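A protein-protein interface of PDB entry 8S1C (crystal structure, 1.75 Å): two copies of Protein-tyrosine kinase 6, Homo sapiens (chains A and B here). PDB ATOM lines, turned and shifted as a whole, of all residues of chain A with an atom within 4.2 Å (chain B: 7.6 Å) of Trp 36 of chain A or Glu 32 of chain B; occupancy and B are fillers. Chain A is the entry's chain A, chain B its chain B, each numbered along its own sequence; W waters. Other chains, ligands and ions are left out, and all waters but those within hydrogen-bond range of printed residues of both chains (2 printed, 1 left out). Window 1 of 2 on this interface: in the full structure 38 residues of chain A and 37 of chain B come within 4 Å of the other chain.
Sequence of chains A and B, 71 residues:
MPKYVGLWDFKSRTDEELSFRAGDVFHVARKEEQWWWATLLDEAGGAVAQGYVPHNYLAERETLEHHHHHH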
ATOM      1  N   TRP A  35      -8.908 -23.908  21.231  1.00  0.00           N
ATOM      2  CA  TRP A  35      -9.815 -24.268  20.160  1.00  0.00           C
ATOM      3  C   TRP A  35     -11.032 -23.370  20.153  1.00  0.00           C
ATOM      4  O   TRP A  35     -11.600 -23.107  21.210  1.00  0.00           O
ATOM      5  CB  TRP A  35     -10.268 -25.713  20.314  1.00  0.00           C
ATOM      6  CG  TRP A  35      -9.138 -26.685  20.146  1.00  0.00           C
ATOM      7  CD1 TRP A  35      -8.247 -27.078  21.100  1.00  0.00           C
ATOM      8  CD2 TRP A  35      -8.761 -27.349  18.935  1.00  0.00           C
ATOM      9  NE1 TRP A  35      -7.339 -27.977  20.543  1.00  0.00           N
ATOM     10  CE2 TRP A  35      -7.650 -28.154  19.222  1.00  0.00           C
ATOM     11  CE3 TRP A  35      -9.279 -27.356  17.639  1.00  0.00           C
ATOM     12  CZ2 TRP A  35      -7.047 -28.950  18.264  1.00  0.00           C
ATOM     13  CZ3 TRP A  35      -8.682 -28.140  16.686  1.00  0.00           C
ATOM     14  CH2 TRP A  35      -7.567 -28.922  16.995  1.00  0.00           C
ATOM     15  N   TRP A  36     -11.457 -22.938  18.958  1.00  0.00           N
ATOM     16  CA  TRP A  36     -12.730 -22.255  18.768  1.00  0.00           C
ATOM     17  C   TRP A  36     -13.619 -23.044  17.817  1.00  0.00           C
ATOM     18  O   TRP A  36     -13.130 -23.618  16.837  1.00  0.00           O
ATOM     19  CB  TRP A  36     -12.577 -20.856  18.152  1.00  0.00           C
ATOM     20  CG  TRP A  36     -11.888 -19.826  18.976  1.00  0.00           C
ATOM     21  CD1 TRP A  36     -11.673 -19.840  20.328  1.00  0.00           C
ATOM     22  CD2 TRP A  36     -11.313 -18.621  18.490  1.00  0.00           C
ATOM     23  NE1 TRP A  36     -10.974 -18.723  20.692  1.00  0.00           N
ATOM     24  CE2 TRP A  36     -10.744 -17.956  19.579  1.00  0.00           C
ATOM     25  CE3 TRP A  36     -11.189 -18.050  17.205  1.00  0.00           C
ATOM     26  CZ2 TRP A  36     -10.104 -16.729  19.447  1.00  0.00           C
ATOM     27  CZ3 TRP A  36     -10.555 -16.843  17.081  1.00  0.00           C
ATOM     28  CH2 TRP A  36     -10.006 -16.198  18.187  1.00  0.00           C
ATOM     29  N   TRP A  37     -14.929 -23.048  18.078  1.00  0.00           N
ATOM     30  CA  TRP A  37     -15.882 -23.435  17.047  1.00  0.00           C
ATOM     31  C   TRP A  37     -15.932 -22.330  16.006  1.00  0.00           C
ATOM     32  O   TRP A  37     -16.055 -21.139  16.347  1.00  0.00           O
ATOM     33  CB  TRP A  37     -17.270 -23.643  17.637  1.00  0.00           C
ATOM     34  CG  TRP A  37     -18.238 -24.266  16.675  1.00  0.00           C
ATOM     35  CD1 TRP A  37     -19.165 -23.627  15.897  1.00  0.00           C
ATOM     36  CD2 TRP A  37     -18.394 -25.654  16.426  1.00  0.00           C
ATOM     37  NE1 TRP A  37     -19.888 -24.557  15.168  1.00  0.00           N
ATOM     38  CE2 TRP A  37     -19.436 -25.805  15.480  1.00  0.00           C
ATOM     39  CE3 TRP A  37     -17.763 -26.796  16.921  1.00  0.00           C
ATOM     40  CZ2 TRP A  37     -19.844 -27.041  15.027  1.00  0.00           C
ATOM     41  CZ3 TRP A  37     -18.164 -28.022  16.460  1.00  0.00           C
ATOM     42  CH2 TRP A  37     -19.188 -28.138  15.508  1.00  0.00           C
ATOM     43  N   ALA A  38     -15.806 -22.708  14.733  1.00  0.00           N
ATOM     44  CA  ALA A  38     -15.731 -21.745  13.647  1.00  0.00           C
ATOM     45  C   ALA A  38     -16.649 -22.155  12.510  1.00  0.00           C
ATOM     46  O   ALA A  38     -16.953 -23.346  12.334  1.00  0.00           O
ATOM     47  CB  ALA A  38     -14.284 -21.610  13.087  1.00  0.00           C
ATOM     48  N   GLY A  51     -16.912 -26.353  12.642  1.00  0.00           N
ATOM     49  CA  GLY A  51     -16.196 -27.289  13.493  1.00  0.00           C
ATOM     50  C   GLY A  51     -15.123 -26.594  14.291  1.00  0.00           C
ATOM     51  O   GLY A  51     -14.922 -25.376  14.189  1.00  0.00           O
ATOM     52  N   TYR A  52     -14.427 -27.389  15.099  1.00  0.00           N
ATOM     53  CA  TYR A  52     -13.387 -26.841  15.957  1.00  0.00           C
ATOM     54  C   TYR A  52     -12.115 -26.592  15.155  1.00  0.00           C
ATOM     55  O   TYR A  52     -11.697 -27.438  14.342  1.00  0.00           O
ATOM     56  CB  TYR A  52     -13.080 -27.789  17.100  1.00  0.00           C
ATOM     57  CG  TYR A  52     -14.141 -27.739  18.169  1.00  0.00           C
ATOM     58  CD1 TYR A  52     -14.292 -26.610  18.954  1.00  0.00           C
ATOM     59  CD2 TYR A  52     -14.989 -28.815  18.378  1.00  0.00           C
ATOM     60  CE1 TYR A  52     -15.245 -26.553  19.934  1.00  0.00           C
ATOM     61  CE2 TYR A  52     -15.961 -28.756  19.356  1.00  0.00           C
ATOM     62  CZ  TYR A  52     -16.075 -27.619  20.125  1.00  0.00           C
ATOM     63  OH  TYR A  52     -17.036 -27.514  21.121  1.00  0.00           O
ATOM     64  N   VAL A  53     -11.515 -25.424  15.374  1.00  0.00           N
ATOM     65  CA  VAL A  53     -10.233 -25.085  14.748  1.00  0.00           C
ATOM     66  C   VAL A  53      -9.311 -24.557  15.844  1.00  0.00           C
ATOM     67  O   VAL A  53      -9.778 -23.988  16.827  1.00  0.00           O
ATOM     68  CB  VAL A  53     -10.404 -24.040  13.641  1.00  0.00           C
ATOM     69  CG1 VAL A  53     -11.310 -24.578  12.553  1.00  0.00           C
ATOM     70  CG2 VAL A  53     -10.969 -22.732  14.187  1.00  0.00           C
ATOM     71  N   HIS A  55      -7.323 -21.789  17.339  1.00  0.00           N
ATOM     72  CA  HIS A  55      -7.513 -20.369  17.016  1.00  0.00           C
ATOM     73  C   HIS A  55      -6.195 -19.676  16.705  1.00  0.00           C
ATOM     74  O   HIS A  55      -6.194 -18.690  15.958  1.00  0.00           O
ATOM     75  CB  HIS A  55      -8.295 -19.637  18.120  1.00  0.00           C
ATOM     76  CG  HIS A  55      -7.548 -19.377  19.398  1.00  0.00           C
ATOM     77  ND1 HIS A  55      -6.597 -18.388  19.519  1.00  0.00           N
ATOM     78  CD2 HIS A  55      -7.670 -19.929  20.627  1.00  0.00           C
ATOM     79  CE1 HIS A  55      -6.130 -18.375  20.752  1.00  0.00           C
ATOM     80  NE2 HIS A  55      -6.765 -19.298  21.448  1.00  0.00           N
ATOM     81  N   PRO B   2     -16.270 -12.226  14.787  1.00  0.00           N
ATOM     82  CA  PRO B   2     -15.470 -11.485  13.812  1.00  0.00           C
ATOM     83  C   PRO B   2     -14.990 -12.409  12.688  1.00  0.00           C
ATOM     84  O   PRO B   2     -15.312 -13.586  12.722  1.00  0.00           O
ATOM     85  CB  PRO B   2     -14.294 -10.966  14.632  1.00  0.00           C
ATOM     86  CG  PRO B   2     -14.867 -10.819  16.012  1.00  0.00           C
ATOM     87  CD  PRO B   2     -15.790 -12.001  16.169  1.00  0.00           C
ATOM     88  N   TYR B   4     -11.830 -14.079  10.361  1.00  0.00           N
ATOM     89  CA  TYR B   4     -10.462 -14.522  10.550  1.00  0.00           C
ATOM     90  C   TYR B   4      -9.956 -15.202   9.290  1.00  0.00           C
ATOM     91  O   TYR B   4     -10.738 -15.739   8.513  1.00  0.00           O
ATOM     92  CB  TYR B   4     -10.370 -15.528  11.693  1.00  0.00           C
ATOM     93  CG  TYR B   4     -10.689 -14.895  13.012  1.00  0.00           C
ATOM     94  CD1 TYR B   4     -12.011 -14.729  13.413  1.00  0.00           C
ATOM     95  CD2 TYR B   4      -9.677 -14.443  13.841  1.00  0.00           C
ATOM     96  CE1 TYR B   4     -12.300 -14.141  14.600  1.00  0.00           C
ATOM     97  CE2 TYR B   4      -9.970 -13.842  15.033  1.00  0.00           C
ATOM     98  CZ  TYR B   4     -11.284 -13.693  15.401  1.00  0.00           C
ATOM     99  OH  TYR B   4     -11.596 -13.091  16.597  1.00  0.00           O
ATOM    100  N   GLU B  16     -15.378 -33.723  14.712  1.00  0.00           N
ATOM    101  CA  GLU B  16     -15.808 -32.410  15.168  1.00  0.00           C
ATOM    102  C   GLU B  16     -14.840 -31.302  14.770  1.00  0.00           C
ATOM    103  O   GLU B  16     -15.234 -30.130  14.741  1.00  0.00           O
ATOM    104  CB  GLU B  16     -15.979 -32.414  16.691  1.00  0.00           C
ATOM    105  CG  GLU B  16     -17.239 -33.104  17.170  1.00  0.00           C
ATOM    106  N   GLU B  17     -13.588 -31.636  14.483  1.00  0.00           N
ATOM    107  CA  GLU B  17     -12.623 -30.629  14.070  1.00  0.00           C
ATOM    108  C   GLU B  17     -12.792 -30.348  12.585  1.00  0.00           C
ATOM    109  O   GLU B  17     -13.307 -31.169  11.839  1.00  0.00           O
ATOM    110  CB  GLU B  17     -11.195 -31.093  14.382  1.00  0.00           C
ATOM    111  CG  GLU B  17     -10.898 -31.056  15.879  1.00  0.00           C
ATOM    112  CD  GLU B  17      -9.674 -31.862  16.305  1.00  0.00           C
ATOM    113  OE1 GLU B  17      -8.948 -32.367  15.441  1.00  0.00           O
ATOM    114  OE2 GLU B  17      -9.434 -31.960  17.525  1.00  0.00           O
ATOM    115  N   LEU B  18     -12.347 -29.166  12.159  1.00  0.00           N
ATOM    116  CA  LEU B  18     -12.571 -28.672  10.803  1.00  0.00           C
ATOM    117  C   LEU B  18     -11.246 -28.438  10.106  1.00  0.00           C
ATOM    118  O   LEU B  18     -10.463 -27.581  10.512  1.00  0.00           O
ATOM    119  CB  LEU B  18     -13.406 -27.387  10.846  1.00  0.00           C
ATOM    120  CG  LEU B  18     -13.681 -26.653   9.551  1.00  0.00           C
ATOM    121  CD1 LEU B  18     -14.426 -27.527   8.542  1.00  0.00           C
ATOM    122  CD2 LEU B  18     -14.458 -25.379   9.837  1.00  0.00           C
ATOM    123  N   PHE B  26     -12.972 -17.448   7.864  1.00  0.00           N
ATOM    124  CA  PHE B  26     -13.907 -17.972   8.845  1.00  0.00           C
ATOM    125  C   PHE B  26     -14.669 -16.840   9.519  1.00  0.00           C
ATOM    126  O   PHE B  26     -14.146 -15.733   9.682  1.00  0.00           O
ATOM    127  CB  PHE B  26     -13.214 -18.714   9.996  1.00  0.00           C
ATOM    128  CG  PHE B  26     -12.351 -19.807   9.568  1.00  0.00           C
ATOM    129  CD1 PHE B  26     -11.064 -19.540   9.104  1.00  0.00           C
ATOM    130  CD2 PHE B  26     -12.802 -21.104   9.577  1.00  0.00           C
ATOM    131  CE1 PHE B  26     -10.257 -20.555   8.679  1.00  0.00           C
ATOM    132  CE2 PHE B  26     -11.972 -22.125   9.112  1.00  0.00           C
ATOM    133  CZ  PHE B  26     -10.712 -21.839   8.684  1.00  0.00           C
ATOM    134  N   HIS B  27     -15.886 -17.155   9.948  1.00  0.00           N
ATOM    135  CA  HIS B  27     -16.599 -16.381  10.957  1.00  0.00           C
ATOM    136  C   HIS B  27     -16.467 -17.109  12.289  1.00  0.00           C
ATOM    137  O   HIS B  27     -16.689 -18.320  12.354  1.00  0.00           O
ATOM    138  CB  HIS B  27     -18.074 -16.229  10.613  1.00  0.00           C
ATOM    139  CG  HIS B  27     -18.880 -15.754  11.787  1.00  0.00           C
ATOM    140  ND1 HIS B  27     -18.856 -14.445  12.217  1.00  0.00           N
ATOM    141  CD2 HIS B  27     -19.663 -16.425  12.662  1.00  0.00           C
ATOM    142  CE1 HIS B  27     -19.609 -14.327  13.298  1.00  0.00           C
ATOM    143  NE2 HIS B  27     -20.118 -15.513  13.583  1.00  0.00           N
ATOM    144  N   VAL B  28     -16.128 -16.376  13.357  1.00  0.00           N
ATOM    145  CA  VAL B  28     -16.081 -16.948  14.694  1.00  0.00           C
ATOM    146  C   VAL B  28     -16.881 -16.037  15.599  1.00  0.00           C
ATOM    147  O   VAL B  28     -16.720 -14.817  15.544  1.00  0.00           O
ATOM    148  CB  VAL B  28     -14.650 -17.075  15.241  1.00  0.00           C
ATOM    149  CG1 VAL B  28     -14.670 -17.778  16.587  1.00  0.00           C
ATOM    150  CG2 VAL B  28     -13.785 -17.796  14.233  1.00  0.00           C
ATOM    151  N   ALA B  29     -17.749 -16.629  16.399  1.00  0.00           N
ATOM    152  CA  ALA B  29     -18.534 -15.852  17.346  1.00  0.00           C
ATOM    153  C   ALA B  29     -17.663 -15.387  18.509  1.00  0.00           C
ATOM    154  O   ALA B  29     -16.762 -16.091  18.955  1.00  0.00           O
ATOM    155  CB  ALA B  29     -19.682 -16.706  17.846  1.00  0.00           C
ATOM    156  N   ARG B  30     -17.930 -14.177  18.994  1.00  0.00           N
ATOM    157  CA  ARG B  30     -17.143 -13.626  20.091  1.00  0.00           C
ATOM    158  C   ARG B  30     -17.124 -14.538  21.311  1.00  0.00           C
ATOM    159  O   ARG B  30     -16.133 -14.562  22.057  1.00  0.00           O
ATOM    160  CB  ARG B  30     -17.709 -12.261  20.515  1.00  0.00           C
ATOM    161  CG  ARG B  30     -17.400 -11.108  19.607  1.00  0.00           C
ATOM    162  CD  ARG B  30     -15.954 -10.665  19.708  1.00  0.00           C
ATOM    163  NE  ARG B  30     -15.601  -9.970  20.943  1.00  0.00           N
ATOM    164  CZ  ARG B  30     -15.967  -8.721  21.225  1.00  0.00           C
ATOM    165  NH1 ARG B  30     -16.789  -8.042  20.433  1.00  0.00           N
ATOM    166  NH2 ARG B  30     -15.502  -8.136  22.326  1.00  0.00           N
ATOM    167  N   LYS B  31     -18.214 -15.269  21.554  1.00  0.00           N
ATOM    168  CA  LYS B  31     -18.306 -16.101  22.748  1.00  0.00           C
ATOM    169  C   LYS B  31     -17.236 -17.173  22.796  1.00  0.00           C
ATOM    170  O   LYS B  31     -16.932 -17.665  23.884  1.00  0.00           O
ATOM    171  CB  LYS B  31     -19.673 -16.780  22.832  1.00  0.00           C
ATOM    172  CG  LYS B  31     -19.972 -17.749  21.698  1.00  0.00           C
ATOM    173  CD  LYS B  31     -21.281 -18.510  21.932  1.00  0.00           C
ATOM    174  CE  LYS B  31     -22.034 -18.697  20.632  1.00  0.00           C
ATOM    175  N   GLU B  32     -16.692 -17.594  21.643  1.00  0.00           N
ATOM    176  CA  GLU B  32     -15.676 -18.640  21.681  1.00  0.00           C
ATOM    177  C   GLU B  32     -14.413 -18.180  22.386  1.00  0.00           C
ATOM    178  O   GLU B  32     -13.705 -18.998  22.979  1.00  0.00           O
ATOM    179  CB  GLU B  32     -15.302 -19.093  20.275  1.00  0.00           C
ATOM    180  CG  GLU B  32     -16.453 -19.677  19.526  1.00  0.00           C
ATOM    181  CD  GLU B  32     -16.935 -20.990  20.096  1.00  0.00           C
ATOM    182  OE1 GLU B  32     -16.099 -21.844  20.447  1.00  0.00           O
ATOM    183  OE2 GLU B  32     -18.169 -21.167  20.194  1.00  0.00           O
ATOM    184  N   GLU B  33     -14.068 -16.897  22.245  1.00  0.00           N
ATOM    185  CA  GLU B  33     -12.933 -16.314  22.921  1.00  0.00           C
ATOM    186  C   GLU B  33     -13.285 -15.875  24.334  1.00  0.00           C
ATOM    187  O   GLU B  33     -12.401 -15.743  25.183  1.00  0.00           O
ATOM    188  CB  GLU B  33     -12.438 -15.106  22.128  1.00  0.00           C
ATOM    189  CG  GLU B  33     -11.045 -14.615  22.514  1.00  0.00           C
ATOM    190  N   GLN B  34     -14.551 -15.644  24.600  1.00  0.00           N
ATOM    191  CA  GLN B  34     -14.912 -15.052  25.879  1.00  0.00           C
ATOM    192  C   GLN B  34     -15.125 -16.068  26.974  1.00  0.00           C
ATOM    193  O   GLN B  34     -15.047 -15.701  28.148  1.00  0.00           O
ATOM    194  CB  GLN B  34     -16.181 -14.215  25.714  1.00  0.00           C
ATOM    195  CG  GLN B  34     -15.895 -12.964  24.900  1.00  0.00           C
ATOM    196  CD  GLN B  34     -17.142 -12.195  24.551  1.00  0.00           C
ATOM    197  OE1 GLN B  34     -18.246 -12.757  24.477  1.00  0.00           O
ATOM    198  NE2 GLN B  34     -16.983 -10.891  24.336  1.00  0.00           N
ATOM    199  N   TRP B  35     -15.403 -17.319  26.644  1.00  0.00           N
ATOM    200  CA  TRP B  35     -15.766 -18.294  27.659  1.00  0.00           C
ATOM    201  C   TRP B  35     -14.859 -19.503  27.581  1.00  0.00           C
ATOM    202  O   TRP B  35     -14.601 -20.021  26.499  1.00  0.00           O
ATOM    203  CB  TRP B  35     -17.222 -18.759  27.512  1.00  0.00           C
ATOM    204  CG  TRP B  35     -18.166 -17.687  27.878  1.00  0.00           C
ATOM    205  CD1 TRP B  35     -18.800 -16.828  27.031  1.00  0.00           C
ATOM    206  CD2 TRP B  35     -18.563 -17.326  29.203  1.00  0.00           C
ATOM    207  NE1 TRP B  35     -19.585 -15.961  27.745  1.00  0.00           N
ATOM    208  CE2 TRP B  35     -19.452 -16.237  29.086  1.00  0.00           C
ATOM    209  CE3 TRP B  35     -18.270 -17.829  30.478  1.00  0.00           C
ATOM    210  CZ2 TRP B  35     -20.060 -15.647  30.195  1.00  0.00           C
ATOM    211  CZ3 TRP B  35     -18.863 -17.225  31.589  1.00  0.00           C
ATOM    212  CH2 TRP B  35     -19.742 -16.147  31.433  1.00  0.00           C
ATOM    213  N   TRP B  36     -14.413 -19.957  28.748  1.00  0.00           N
ATOM    214  CA  TRP B  36     -13.532 -21.103  28.891  1.00  0.00           C
ATOM    215  C   TRP B  36     -14.121 -22.087  29.894  1.00  0.00           C
ATOM    216  O   TRP B  36     -14.534 -21.689  30.990  1.00  0.00           O
ATOM    217  CB  TRP B  36     -12.177 -20.672  29.414  1.00  0.00           C
ATOM    218  CG  TRP B  36     -11.226 -20.030  28.462  1.00  0.00           C
ATOM    219  CD1 TRP B  36     -11.392 -19.799  27.118  1.00  0.00           C
ATOM    220  CD2 TRP B  36      -9.933 -19.541  28.801  1.00  0.00           C
ATOM    221  NE1 TRP B  36     -10.246 -19.211  26.602  1.00  0.00           N
ATOM    222  CE2 TRP B  36      -9.346 -19.038  27.623  1.00  0.00           C
ATOM    223  CE3 TRP B  36      -9.201 -19.479  30.006  1.00  0.00           C
ATOM    224  CZ2 TRP B  36      -8.059 -18.495  27.613  1.00  0.00           C
ATOM    225  CZ3 TRP B  36      -7.946 -18.947  29.986  1.00  0.00           C
ATOM    226  CH2 TRP B  36      -7.378 -18.460  28.799  1.00  0.00           C
ATOM    227  N   HIS B  55     -12.938 -16.008  30.131  1.00  0.00           N
ATOM    228  CA  HIS B  55     -11.519 -15.981  29.808  1.00  0.00           C
ATOM    229  C   HIS B  55     -10.858 -14.763  30.399  1.00  0.00           C
ATOM    230  O   HIS B  55      -9.811 -14.847  31.039  1.00  0.00           O
ATOM    231  CB  HIS B  55     -11.433 -16.010  28.278  1.00  0.00           C
ATOM    232  CG  HIS B  55     -10.090 -15.700  27.704  1.00  0.00           C
ATOM    233  ND1 HIS B  55      -9.881 -15.697  26.339  1.00  0.00           N
ATOM    234  CD2 HIS B  55      -8.897 -15.408  28.272  1.00  0.00           C
ATOM    235  CE1 HIS B  55      -8.614 -15.409  26.092  1.00  0.00           C
ATOM    236  NE2 HIS B  55      -7.995 -15.227  27.247  1.00  0.00           N
HETATM  237  O   HOH W   1     -18.295 -19.463  16.163  1.00  0.00           O
HETATM  238  O   HOH W   2     -11.352 -20.735  23.677  1.00  0.00           O
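OE1 of Glu 32 of chain B sits at hydrogen-bond distance from N of Trp 37 of chain A (2.9 Å).
N of Leu 18 of chain B is in hydrogen-bond range of O of Tyr 52 of chain A (2.9 Å).
The backbone NH (N) of Tyr 52 of chain A is in hydrogen-bond range of the backbone carbonyl oxygen (O) of Glu 16 of chain B (2.9 Å).
The backbone carbonyl oxygen (O) of Trp 36 of chain A sits at hydrogen-bond distance from the backbone NH (N) of Val 53 of chain A (2.8 Å).
The backbone carbonyl oxygen (O) of Tyr 4 of chain B sits at hydrogen-bond distance from the backbone NH (N) of Phe 26 of chain B (2.9 Å).
A ring nitrogen (ND1) of His 55 of chain B is in hydrogen-bond range of the backbone carbonyl oxygen (O) of Glu 33 of chain B (2.8 Å).
The backbone carbonyl oxygen (O) of Gly 51 of chain A sits at hydrogen-bond distance from the backbone NH (N) of Ala 38 of chain A (2.9 Å).
The backbone carbonyl oxygen of Pro 2 of chain B is in hydrogen-bond range of the backbone NH of Val 28 of chain B (3.0 Å).
OE2 of Glu 17 of chain B touches CH2 of Trp 35 of chain A, 3.6 Å away.
CZ3 of Trp 36 of chain A touches CZ of Tyr 4 of chain B, 3.6 Å away.
Val 28 of chain B touches Trp 36 of chain A.
Trp 36 of chain A touches Glu 32 of chain B.
Glu 16 of chain B touches Trp 37 of chain A (O to CZ3, 3.998 Å).
CG1 of Val 28 of chain B touches O of Trp 37 of chain A (3.6 Å).
Phe 26 of chain B touches Ala 38 of chain A (CD2 to CB, 3.8 Å).
His 27 of chain B touches Ala 38 of chain A.
Gly 51 of chain A touches Leu 18 of chain B (CA to CB, 3.8 Å).
CA of Glu 17 of chain B touches O of Tyr 52 of chain A (3.3 Å).
Of the printed residues of chain B, Trp 36 of chain A touches Tyr 4, Val 28, Glu 32 and Glu 33.
Glu 32 of chain B touches just these residues of chain A: Trp 36 (3.4 Å) and Trp 37 (2.9 Å).
Printed residues of chain A within 4 Å of Tyr 4 of chain B: Trp 36.
Of the printed residues of chain B, Val 53 of chain A touches Leu 18 (3.7 Å).
Of the printed residues of chain A, Leu 18 of chain B touches Gly 51 (3.8 Å), Tyr 52 (2.9 Å) and Val 53 (3.7 Å).
Printed residues of chain B within 4 Å of Gly 51 of chain A: Glu 16 (3.2 Å) and Leu 18 (3.8 Å).
Lys 31 of chain B touches none of the printed residues of chain A.
The nearest printed residue of chain A that does not touch Glu 32 of chain B is Trp 35 of chain A (4.7 Å).
The nearest printed residue of chain B that does not touch Ala 38 of chain A is Val 28 of chain B (4.01 Å).
Of the 8 printed residues of chain A, 7 touch a printed residue of chain B.
Among the printed residues, no Asp or Glu carboxylate lies within 4 Å of a Lys or Arg side-chain nitrogen of the other chain.
Positions printed for both chains: 35, 36 and 55.
Of the 16 pairs that touch across the chains among the printed residues, none has its exchanged pair printed and touching as well.
Water W1 bridges O of Trp 37 of chain A and N of Ala 29 of chain B.
Water W2 lies within hydrogen-bond range of the backbone carbonyl oxygen (O) of Glu 32 of chain B, the backbone carbonyl oxygen (O) of Trp 35 of chain A and the indole nitrogen (NE1) of Trp 36 of chain B.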
